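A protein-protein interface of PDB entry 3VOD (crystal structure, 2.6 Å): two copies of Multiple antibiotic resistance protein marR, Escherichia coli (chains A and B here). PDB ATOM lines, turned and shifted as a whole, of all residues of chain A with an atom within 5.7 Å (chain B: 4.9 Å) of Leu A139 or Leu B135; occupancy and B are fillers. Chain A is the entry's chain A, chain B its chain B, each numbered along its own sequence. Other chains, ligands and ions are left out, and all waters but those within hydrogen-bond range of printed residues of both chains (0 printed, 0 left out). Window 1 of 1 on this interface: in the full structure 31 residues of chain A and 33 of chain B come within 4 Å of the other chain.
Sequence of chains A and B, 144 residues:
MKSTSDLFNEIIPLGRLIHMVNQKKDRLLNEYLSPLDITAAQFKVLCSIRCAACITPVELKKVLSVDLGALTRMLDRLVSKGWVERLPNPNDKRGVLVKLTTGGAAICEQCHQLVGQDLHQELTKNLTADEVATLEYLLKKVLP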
ATOM      1  N   LEU A  14       4.879  -5.552  13.666  1.00  0.00           N
ATOM      2  CA  LEU A  14       5.668  -4.462  14.236  1.00  0.00           C
ATOM      3  C   LEU A  14       6.559  -4.887  15.400  1.00  0.00           C
ATOM      4  O   LEU A  14       7.722  -4.488  15.472  1.00  0.00           O
ATOM      5  CB  LEU A  14       4.747  -3.324  14.684  1.00  0.00           C
ATOM      6  CG  LEU A  14       5.447  -2.006  15.020  1.00  0.00           C
ATOM      7  CD1 LEU A  14       6.082  -1.398  13.774  1.00  0.00           C
ATOM      8  CD2 LEU A  14       4.497  -1.021  15.684  1.00  0.00           C
ATOM      9  N   LEU A  17       9.611  -6.881  14.117  1.00  0.00           N
ATOM     10  CA  LEU A  17      10.438  -5.974  13.318  1.00  0.00           C
ATOM     11  C   LEU A  17      11.319  -5.102  14.199  1.00  0.00           C
ATOM     12  O   LEU A  17      12.524  -5.001  13.964  1.00  0.00           O
ATOM     13  CB  LEU A  17       9.580  -5.085  12.412  1.00  0.00           C
ATOM     14  CG  LEU A  17       8.993  -5.691  11.133  1.00  0.00           C
ATOM     15  CD1 LEU A  17       8.114  -4.663  10.437  1.00  0.00           C
ATOM     16  CD2 LEU A  17      10.074  -6.208  10.191  1.00  0.00           C
ATOM     17  N   ILE A  18      10.710  -4.482  15.210  1.00  0.00           N
ATOM     18  CA  ILE A  18      11.440  -3.651  16.159  1.00  0.00           C
ATOM     19  C   ILE A  18      12.524  -4.452  16.878  1.00  0.00           C
ATOM     20  O   ILE A  18      13.618  -3.940  17.094  1.00  0.00           O
ATOM     21  CB  ILE A  18      10.488  -2.931  17.140  1.00  0.00           C
ATOM     22  CG1 ILE A  18       9.940  -1.660  16.488  1.00  0.00           C
ATOM     23  CG2 ILE A  18      11.181  -2.576  18.450  1.00  0.00           C
ATOM     24  CD1 ILE A  18       8.467  -1.435  16.755  1.00  0.00           C
ATOM     25  N   THR A 134      10.591  10.176   7.592  1.00  0.00           N
ATOM     26  CA  THR A 134       9.311   9.484   7.789  1.00  0.00           C
ATOM     27  C   THR A 134       9.422   8.372   8.836  1.00  0.00           C
ATOM     28  O   THR A 134       8.525   8.211   9.673  1.00  0.00           O
ATOM     29  CB  THR A 134       8.763   8.903   6.465  1.00  0.00           C
ATOM     30  OG1 THR A 134       8.606   9.957   5.509  1.00  0.00           O
ATOM     31  CG2 THR A 134       7.403   8.214   6.674  1.00  0.00           C
ATOM     32  N   LEU A 135      10.522   7.617   8.794  1.00  0.00           N
ATOM     33  CA  LEU A 135      10.744   6.533   9.751  1.00  0.00           C
ATOM     34  C   LEU A 135      10.817   7.041  11.194  1.00  0.00           C
ATOM     35  O   LEU A 135      10.158   6.489  12.077  1.00  0.00           O
ATOM     36  CB  LEU A 135      11.991   5.724   9.392  1.00  0.00           C
ATOM     37  CG  LEU A 135      12.364   4.536  10.292  1.00  0.00           C
ATOM     38  CD1 LEU A 135      11.178   3.620  10.617  1.00  0.00           C
ATOM     39  CD2 LEU A 135      13.504   3.759   9.650  1.00  0.00           C
ATOM     40  N   GLU A 136      11.606   8.088  11.426  1.00  0.00           N
ATOM     41  CA  GLU A 136      11.726   8.676  12.759  1.00  0.00           C
ATOM     42  C   GLU A 136      10.406   9.254  13.248  1.00  0.00           C
ATOM     43  O   GLU A 136      10.056   9.097  14.420  1.00  0.00           O
ATOM     44  CB  GLU A 136      12.808   9.748  12.788  1.00  0.00           C
ATOM     45  CG  GLU A 136      14.226   9.186  12.825  1.00  0.00           C
ATOM     46  CD  GLU A 136      15.288  10.251  12.603  1.00  0.00           C
ATOM     47  OE1 GLU A 136      14.952  11.369  12.143  1.00  0.00           O
ATOM     48  OE2 GLU A 136      16.470   9.964  12.891  1.00  0.00           O
ATOM     49  N   TYR A 137       9.675   9.907  12.344  1.00  0.00           N
ATOM     50  CA  TYR A 137       8.392  10.528  12.672  1.00  0.00           C
ATOM     51  C   TYR A 137       7.363   9.510  13.191  1.00  0.00           C
ATOM     52  O   TYR A 137       6.646   9.775  14.165  1.00  0.00           O
ATOM     53  CB  TYR A 137       7.847  11.280  11.450  1.00  0.00           C
ATOM     54  CG  TYR A 137       6.407  11.738  11.587  1.00  0.00           C
ATOM     55  CD1 TYR A 137       6.058  12.752  12.483  1.00  0.00           C
ATOM     56  CD2 TYR A 137       5.394  11.157  10.819  1.00  0.00           C
ATOM     57  CE1 TYR A 137       4.744  13.172  12.615  1.00  0.00           C
ATOM     58  CE2 TYR A 137       4.079  11.575  10.940  1.00  0.00           C
ATOM     59  CZ  TYR A 137       3.764  12.581  11.839  1.00  0.00           C
ATOM     60  OH  TYR A 137       2.468  12.994  11.964  1.00  0.00           O
ATOM     61  N   LEU A 138       7.298   8.351  12.537  1.00  0.00           N
ATOM     62  CA  LEU A 138       6.348   7.307  12.907  1.00  0.00           C
ATOM     63  C   LEU A 138       6.787   6.559  14.162  1.00  0.00           C
ATOM     64  O   LEU A 138       5.947   6.157  14.965  1.00  0.00           O
ATOM     65  CB  LEU A 138       6.115   6.336  11.741  1.00  0.00           C
ATOM     66  CG  LEU A 138       5.547   6.914  10.435  1.00  0.00           C
ATOM     67  CD1 LEU A 138       5.594   5.882   9.316  1.00  0.00           C
ATOM     68  CD2 LEU A 138       4.131   7.443  10.613  1.00  0.00           C
ATOM     69  N   LEU A 139       8.095   6.369  14.335  1.00  0.00           N
ATOM     70  CA  LEU A 139       8.607   5.756  15.563  1.00  0.00           C
ATOM     71  C   LEU A 139       8.261   6.597  16.798  1.00  0.00           C
ATOM     72  O   LEU A 139       7.785   6.058  17.800  1.00  0.00           O
ATOM     73  CB  LEU A 139      10.112   5.498  15.483  1.00  0.00           C
ATOM     74  CG  LEU A 139      10.614   4.369  14.574  1.00  0.00           C
ATOM     75  CD1 LEU A 139      12.130   4.395  14.511  1.00  0.00           C
ATOM     76  CD2 LEU A 139      10.127   3.001  15.032  1.00  0.00           C
ATOM     77  N   LYS A 140       8.481   7.913  16.708  1.00  0.00           N
ATOM     78  CA  LYS A 140       8.085   8.859  17.759  1.00  0.00           C
ATOM     79  C   LYS A 140       6.606   8.694  18.141  1.00  0.00           C
ATOM     80  O   LYS A 140       6.261   8.766  19.321  1.00  0.00           O
ATOM     81  CB  LYS A 140       8.329  10.306  17.314  1.00  0.00           C
ATOM     82  CG  LYS A 140       9.789  10.717  17.151  1.00  0.00           C
ATOM     83  CD  LYS A 140       9.952  12.221  17.358  1.00  0.00           C
ATOM     84  CE  LYS A 140      11.252  12.723  16.743  1.00  0.00           C
ATOM     85  NZ  LYS A 140      11.059  13.221  15.346  1.00  0.00           N
ATOM     86  N   LYS A 141       5.749   8.463  17.143  1.00  0.00           N
ATOM     87  CA  LYS A 141       4.306   8.288  17.364  1.00  0.00           C
ATOM     88  C   LYS A 141       3.951   7.088  18.240  1.00  0.00           C
ATOM     89  O   LYS A 141       2.911   7.079  18.886  1.00  0.00           O
ATOM     90  CB  LYS A 141       3.548   8.200  16.037  1.00  0.00           C
ATOM     91  CG  LYS A 141       3.325   9.546  15.371  1.00  0.00           C
ATOM     92  CD  LYS A 141       2.249   9.481  14.302  1.00  0.00           C
ATOM     93  CE  LYS A 141       1.535  10.817  14.204  1.00  0.00           C
ATOM     94  NZ  LYS A 141       0.668  10.909  12.994  1.00  0.00           N
ATOM     95  N   VAL A 142       4.823   6.090  18.256  1.00  0.00           N
ATOM     96  CA  VAL A 142       4.634   4.884  19.057  1.00  0.00           C
ATOM     97  C   VAL A 142       4.948   5.151  20.539  1.00  0.00           C
ATOM     98  O   VAL A 142       4.525   4.392  21.409  1.00  0.00           O
ATOM     99  CB  VAL A 142       5.510   3.717  18.511  1.00  0.00           C
ATOM    100  CG1 VAL A 142       5.321   2.436  19.315  1.00  0.00           C
ATOM    101  CG2 VAL A 142       5.187   3.441  17.053  1.00  0.00           C
ATOM    102  N   LEU A 143       5.664   6.239  20.826  1.00  0.00           N
ATOM    103  CA  LEU A 143       6.206   6.465  22.175  1.00  0.00           C
ATOM    104  C   LEU A 143       5.318   7.134  23.246  1.00  0.00           C
ATOM    105  O   LEU A 143       5.540   6.917  24.445  1.00  0.00           O
ATOM    106  CB  LEU A 143       7.569   7.154  22.095  1.00  0.00           C
ATOM    107  CG  LEU A 143       8.690   6.247  21.587  1.00  0.00           C
ATOM    108  CD1 LEU A 143       9.949   7.062  21.333  1.00  0.00           C
ATOM    109  CD2 LEU A 143       8.953   5.100  22.555  1.00  0.00           C
ATOM    110  N   LEU B  14      17.713   7.927  15.025  1.00  0.00           N
ATOM    111  CA  LEU B  14      17.039   6.651  14.779  1.00  0.00           C
ATOM    112  C   LEU B  14      17.383   5.559  15.795  1.00  0.00           C
ATOM    113  O   LEU B  14      16.495   4.849  16.274  1.00  0.00           O
ATOM    114  CB  LEU B  14      17.328   6.158  13.354  1.00  0.00           C
ATOM    115  CG  LEU B  14      16.554   4.921  12.887  1.00  0.00           C
ATOM    116  CD1 LEU B  14      15.069   5.218  12.798  1.00  0.00           C
ATOM    117  CD2 LEU B  14      17.069   4.408  11.555  1.00  0.00           C
ATOM    118  N   LEU B  17      15.541   5.997  19.176  1.00  0.00           N
ATOM    119  CA  LEU B  17      14.108   5.777  18.981  1.00  0.00           C
ATOM    120  C   LEU B  17      13.780   4.293  18.925  1.00  0.00           C
ATOM    121  O   LEU B  17      12.843   3.838  19.578  1.00  0.00           O
ATOM    122  CB  LEU B  17      13.611   6.462  17.704  1.00  0.00           C
ATOM    123  CG  LEU B  17      13.414   7.981  17.712  1.00  0.00           C
ATOM    124  CD1 LEU B  17      12.944   8.419  16.332  1.00  0.00           C
ATOM    125  CD2 LEU B  17      12.430   8.432  18.792  1.00  0.00           C
ATOM    126  N   ILE B  18      14.557   3.544  18.150  1.00  0.00           N
ATOM    127  CA  ILE B  18      14.410   2.096  18.090  1.00  0.00           C
ATOM    128  C   ILE B  18      14.577   1.458  19.472  1.00  0.00           C
ATOM    129  O   ILE B  18      13.784   0.593  19.846  1.00  0.00           O
ATOM    130  CB  ILE B  18      15.342   1.476  17.024  1.00  0.00           C
ATOM    131  CG1 ILE B  18      14.645   1.521  15.664  1.00  0.00           C
ATOM    132  CG2 ILE B  18      15.688   0.032  17.359  1.00  0.00           C
ATOM    133  CD1 ILE B  18      15.579   1.733  14.495  1.00  0.00           C
ATOM    134  N   VAL B  21      11.363   2.439  21.643  1.00  0.00           N
ATOM    135  CA  VAL B  21      10.208   1.672  21.157  1.00  0.00           C
ATOM    136  C   VAL B  21      10.317   0.182  21.515  1.00  0.00           C
ATOM    137  O   VAL B  21       9.312  -0.448  21.870  1.00  0.00           O
ATOM    138  CB  VAL B  21       9.977   1.861  19.639  1.00  0.00           C
ATOM    139  CG1 VAL B  21       8.816   1.005  19.159  1.00  0.00           C
ATOM    140  CG2 VAL B  21       9.692   3.322  19.319  1.00  0.00           C
ATOM    141  N   LEU B 127      -1.435   5.419  15.799  1.00  0.00           N
ATOM    142  CA  LEU B 127      -1.149   5.416  14.372  1.00  0.00           C
ATOM    143  C   LEU B 127      -2.314   4.894  13.560  1.00  0.00           C
ATOM    144  O   LEU B 127      -3.036   3.996  13.997  1.00  0.00           O
ATOM    145  CB  LEU B 127       0.063   4.529  14.088  1.00  0.00           C
ATOM    146  CG  LEU B 127       1.443   4.997  14.533  1.00  0.00           C
ATOM    147  CD1 LEU B 127       2.345   3.786  14.686  1.00  0.00           C
ATOM    148  CD2 LEU B 127       2.030   5.968  13.525  1.00  0.00           C
ATOM    149  N   GLU B 131      -0.436   4.539   8.417  1.00  0.00           N
ATOM    150  CA  GLU B 131       0.887   4.835   8.965  1.00  0.00           C
ATOM    151  C   GLU B 131       1.579   3.581   9.477  1.00  0.00           C
ATOM    152  O   GLU B 131       2.805   3.489   9.438  1.00  0.00           O
ATOM    153  CB  GLU B 131       0.777   5.851  10.099  1.00  0.00           C
ATOM    154  CG  GLU B 131       0.415   7.264   9.662  1.00  0.00           C
ATOM    155  CD  GLU B 131      -0.030   8.141  10.823  1.00  0.00           C
ATOM    156  OE1 GLU B 131       0.443   9.293  10.913  1.00  0.00           O
ATOM    157  OE2 GLU B 131      -0.851   7.684  11.646  1.00  0.00           O
ATOM    158  N   VAL B 132       0.789   2.621   9.961  1.00  0.00           N
ATOM    159  CA  VAL B 132       1.305   1.320  10.398  1.00  0.00           C
ATOM    160  C   VAL B 132       2.027   0.612   9.242  1.00  0.00           C
ATOM    161  O   VAL B 132       3.108   0.043   9.423  1.00  0.00           O
ATOM    162  CB  VAL B 132       0.177   0.412  10.960  1.00  0.00           C
ATOM    163  CG1 VAL B 132       0.680  -1.007  11.199  1.00  0.00           C
ATOM    164  CG2 VAL B 132      -0.372   0.978  12.263  1.00  0.00           C
ATOM    165  N   ALA B 133       1.421   0.667   8.057  1.00  0.00           N
ATOM    166  CA  ALA B 133       1.947   0.018   6.868  1.00  0.00           C
ATOM    167  C   ALA B 133       3.269   0.642   6.464  1.00  0.00           C
ATOM    168  O   ALA B 133       4.236  -0.070   6.192  1.00  0.00           O
ATOM    169  CB  ALA B 133       0.940   0.101   5.729  1.00  0.00           C
ATOM    170  N   THR B 134       3.309   1.972   6.450  1.00  0.00           N
ATOM    171  CA  THR B 134       4.525   2.711   6.105  1.00  0.00           C
ATOM    172  C   THR B 134       5.656   2.378   7.086  1.00  0.00           C
ATOM    173  O   THR B 134       6.790   2.125   6.668  1.00  0.00           O
ATOM    174  CB  THR B 134       4.276   4.236   6.084  1.00  0.00           C
ATOM    175  OG1 THR B 134       3.057   4.512   5.383  1.00  0.00           O
ATOM    176  CG2 THR B 134       5.424   4.971   5.405  1.00  0.00           C
ATOM    177  N   LEU B 135       5.335   2.379   8.382  1.00  0.00           N
ATOM    178  CA  LEU B 135       6.303   2.063   9.432  1.00  0.00           C
ATOM    179  C   LEU B 135       6.901   0.669   9.252  1.00  0.00           C
ATOM    180  O   LEU B 135       8.124   0.500   9.299  1.00  0.00           O
ATOM    181  CB  LEU B 135       5.659   2.193  10.814  1.00  0.00           C
ATOM    182  CG  LEU B 135       6.525   1.984  12.062  1.00  0.00           C
ATOM    183  CD1 LEU B 135       7.745   2.899  12.072  1.00  0.00           C
ATOM    184  CD2 LEU B 135       5.691   2.196  13.318  1.00  0.00           C
ATOM    185  N   GLU B 136       6.039  -0.324   9.042  1.00  0.00           N
ATOM    186  CA  GLU B 136       6.491  -1.697   8.805  1.00  0.00           C
ATOM    187  C   GLU B 136       7.379  -1.788   7.557  1.00  0.00           C
ATOM    188  O   GLU B 136       8.429  -2.429   7.580  1.00  0.00           O
ATOM    189  CB  GLU B 136       5.294  -2.651   8.707  1.00  0.00           C
ATOM    190  CG  GLU B 136       4.634  -2.946  10.055  1.00  0.00           C
ATOM    191  CD  GLU B 136       3.387  -3.816   9.950  1.00  0.00           C
ATOM    192  OE1 GLU B 136       3.027  -4.263   8.835  1.00  0.00           O
ATOM    193  OE2 GLU B 136       2.757  -4.061  11.006  1.00  0.00           O
ATOM    194  N   TYR B 137       6.953  -1.120   6.488  1.00  0.00           N
ATOM    195  CA  TYR B 137       7.689  -1.046   5.230  1.00  0.00           C
ATOM    196  C   TYR B 137       9.111  -0.483   5.367  1.00  0.00           C
ATOM    197  O   TYR B 137      10.064  -1.054   4.824  1.00  0.00           O
ATOM    198  CB  TYR B 137       6.883  -0.231   4.207  1.00  0.00           C
ATOM    199  CG  TYR B 137       7.635   0.095   2.936  1.00  0.00           C
ATOM    200  CD1 TYR B 137       8.024  -0.915   2.058  1.00  0.00           C
ATOM    201  CD2 TYR B 137       7.954   1.414   2.608  1.00  0.00           C
ATOM    202  CE1 TYR B 137       8.714  -0.629   0.895  1.00  0.00           C
ATOM    203  CE2 TYR B 137       8.644   1.712   1.442  1.00  0.00           C
ATOM    204  CZ  TYR B 137       9.021   0.682   0.593  1.00  0.00           C
ATOM    205  OH  TYR B 137       9.706   0.952  -0.564  1.00  0.00           O
ATOM    206  N   LEU B 138       9.247   0.632   6.085  1.00  0.00           N
ATOM    207  CA  LEU B 138      10.542   1.314   6.220  1.00  0.00           C
ATOM    208  C   LEU B 138      11.480   0.618   7.203  1.00  0.00           C
ATOM    209  O   LEU B 138      12.699   0.661   7.040  1.00  0.00           O
ATOM    210  CB  LEU B 138      10.345   2.781   6.610  1.00  0.00           C
ATOM    211  CG  LEU B 138       9.579   3.682   5.634  1.00  0.00           C
ATOM    212  CD1 LEU B 138       9.387   5.057   6.244  1.00  0.00           C
ATOM    213  CD2 LEU B 138      10.270   3.788   4.280  1.00  0.00           C
ATOM    214  N   LEU B 139      10.906  -0.018   8.224  1.00  0.00           N
ATOM    215  CA  LEU B 139      11.680  -0.853   9.137  1.00  0.00           C
ATOM    216  C   LEU B 139      12.249  -2.077   8.424  1.00  0.00           C
ATOM    217  O   LEU B 139      13.389  -2.482   8.692  1.00  0.00           O
ATOM    218  CB  LEU B 139      10.845  -1.282  10.338  1.00  0.00           C
ATOM    219  CG  LEU B 139      10.661  -0.258  11.461  1.00  0.00           C
ATOM    220  CD1 LEU B 139       9.680  -0.799  12.491  1.00  0.00           C
ATOM    221  CD2 LEU B 139      11.989   0.130  12.113  1.00  0.00           C
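The side-chain amino group (NZ) of Lys A141 is in salt-bridge range of the side-chain carboxylate (OE1) of Glu B131 (2.6 Å).
The side-chain carboxylate (OE2) of Glu A136 sits at hydrogen-bond distance from the backbone NH (N) of Leu B14, at 3.2 Å.
NZ of Lys A141 is in hydrogen-bond range of OH of Tyr A137 (2.9 Å).
CD1 of Leu A17 touches O of Glu B136, at 3.6 Å.
CD1 of Leu B138 touches CG2 of Thr A134, at 3.8 Å.
Glu A136 touches Leu B17 (O to CD1, 3.5 Å).
CD1 of Leu A138 touches O of Glu B131 (3.7 Å).
Leu A138 touches Thr B134.
Leu A139 touches Leu B14 (CD1 to CD1, 3.5 Å).
O of Leu A139 touches CG2 of Val B21, at 3.7 Å.
CG of Lys A140 touches CD2 of Leu B17, 3.9 Å away.
Lys A141 touches Leu B127.
Leu A143 touches Leu B17.
Printed residues of chain B within 4 Å of Leu A139: Leu B14 (3.5 Å), Ile B18 (3.99 Å), Val B21 (3.7 Å) and Leu B135 (3.8 Å).
Of chain A, only Leu A14 (3.6 Å), Leu A135 (3.8 Å), Leu A138 (3.6 Å), Leu A139 (3.8 Å) and Val A142 (3.97 Å) come within 4 Å of Leu B135.
Of the printed residues of chain B, Lys A140 touches Leu B17.
Of the printed residues of chain B, Leu A14 touches Leu B135 (3.6 Å), Glu B136 (3.7 Å) and Leu B139 (3.9 Å).
Of the printed residues of chain B, Thr A134 touches Leu B138 (3.8 Å).
Printed residues of chain A within 4 Å of Leu B138: Thr A134 (3.8 Å) and Leu A135 (3.8 Å).
Tyr A137 touches none of the printed residues of chain B.
The nearest printed residue of chain B that does not touch Leu A139 is Leu B17 (4.1 Å).
The nearest residue of chain A that does not touch Leu B135 is Leu A17 (5.3 Å).
Hydrophobic or aromatic side chains of chain A that line the printed part of chain B: Leu A14, Leu A17, Ile A18, Leu A135, Leu A138, Leu A139, Val A142 and Leu A143.
Printed residues of chain B that touch a printed residue of chain A: Leu B14, Leu B17, Ile B18, Val B21, Leu B127, Glu B131, Thr B134, Leu B135, Glu B136, Leu B138 and Leu B139.
Hydrophobic or aromatic side chains of chain B that line the printed part of chain A: Leu B14, Leu B17, Ile B18, Val B21, Leu B127, Leu B135, Leu B138 and Leu B139.
Leu A14 touches Leu B135, and with the chains exchanged Leu A135 touches Leu B14.
Leu A14 touches Glu B136, and with the chains exchanged Glu A136 touches Leu B14.
Leu A17 touches Glu B136, and with the chains exchanged Glu A136 touches Leu B17.
Thr A134 touches Leu B138, and with the chains exchanged Leu A138 touches Thr B134.
Of the 28 pairs that touch across the chains among the printed residues, 15 have their exchanged pair printed and touching as well.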
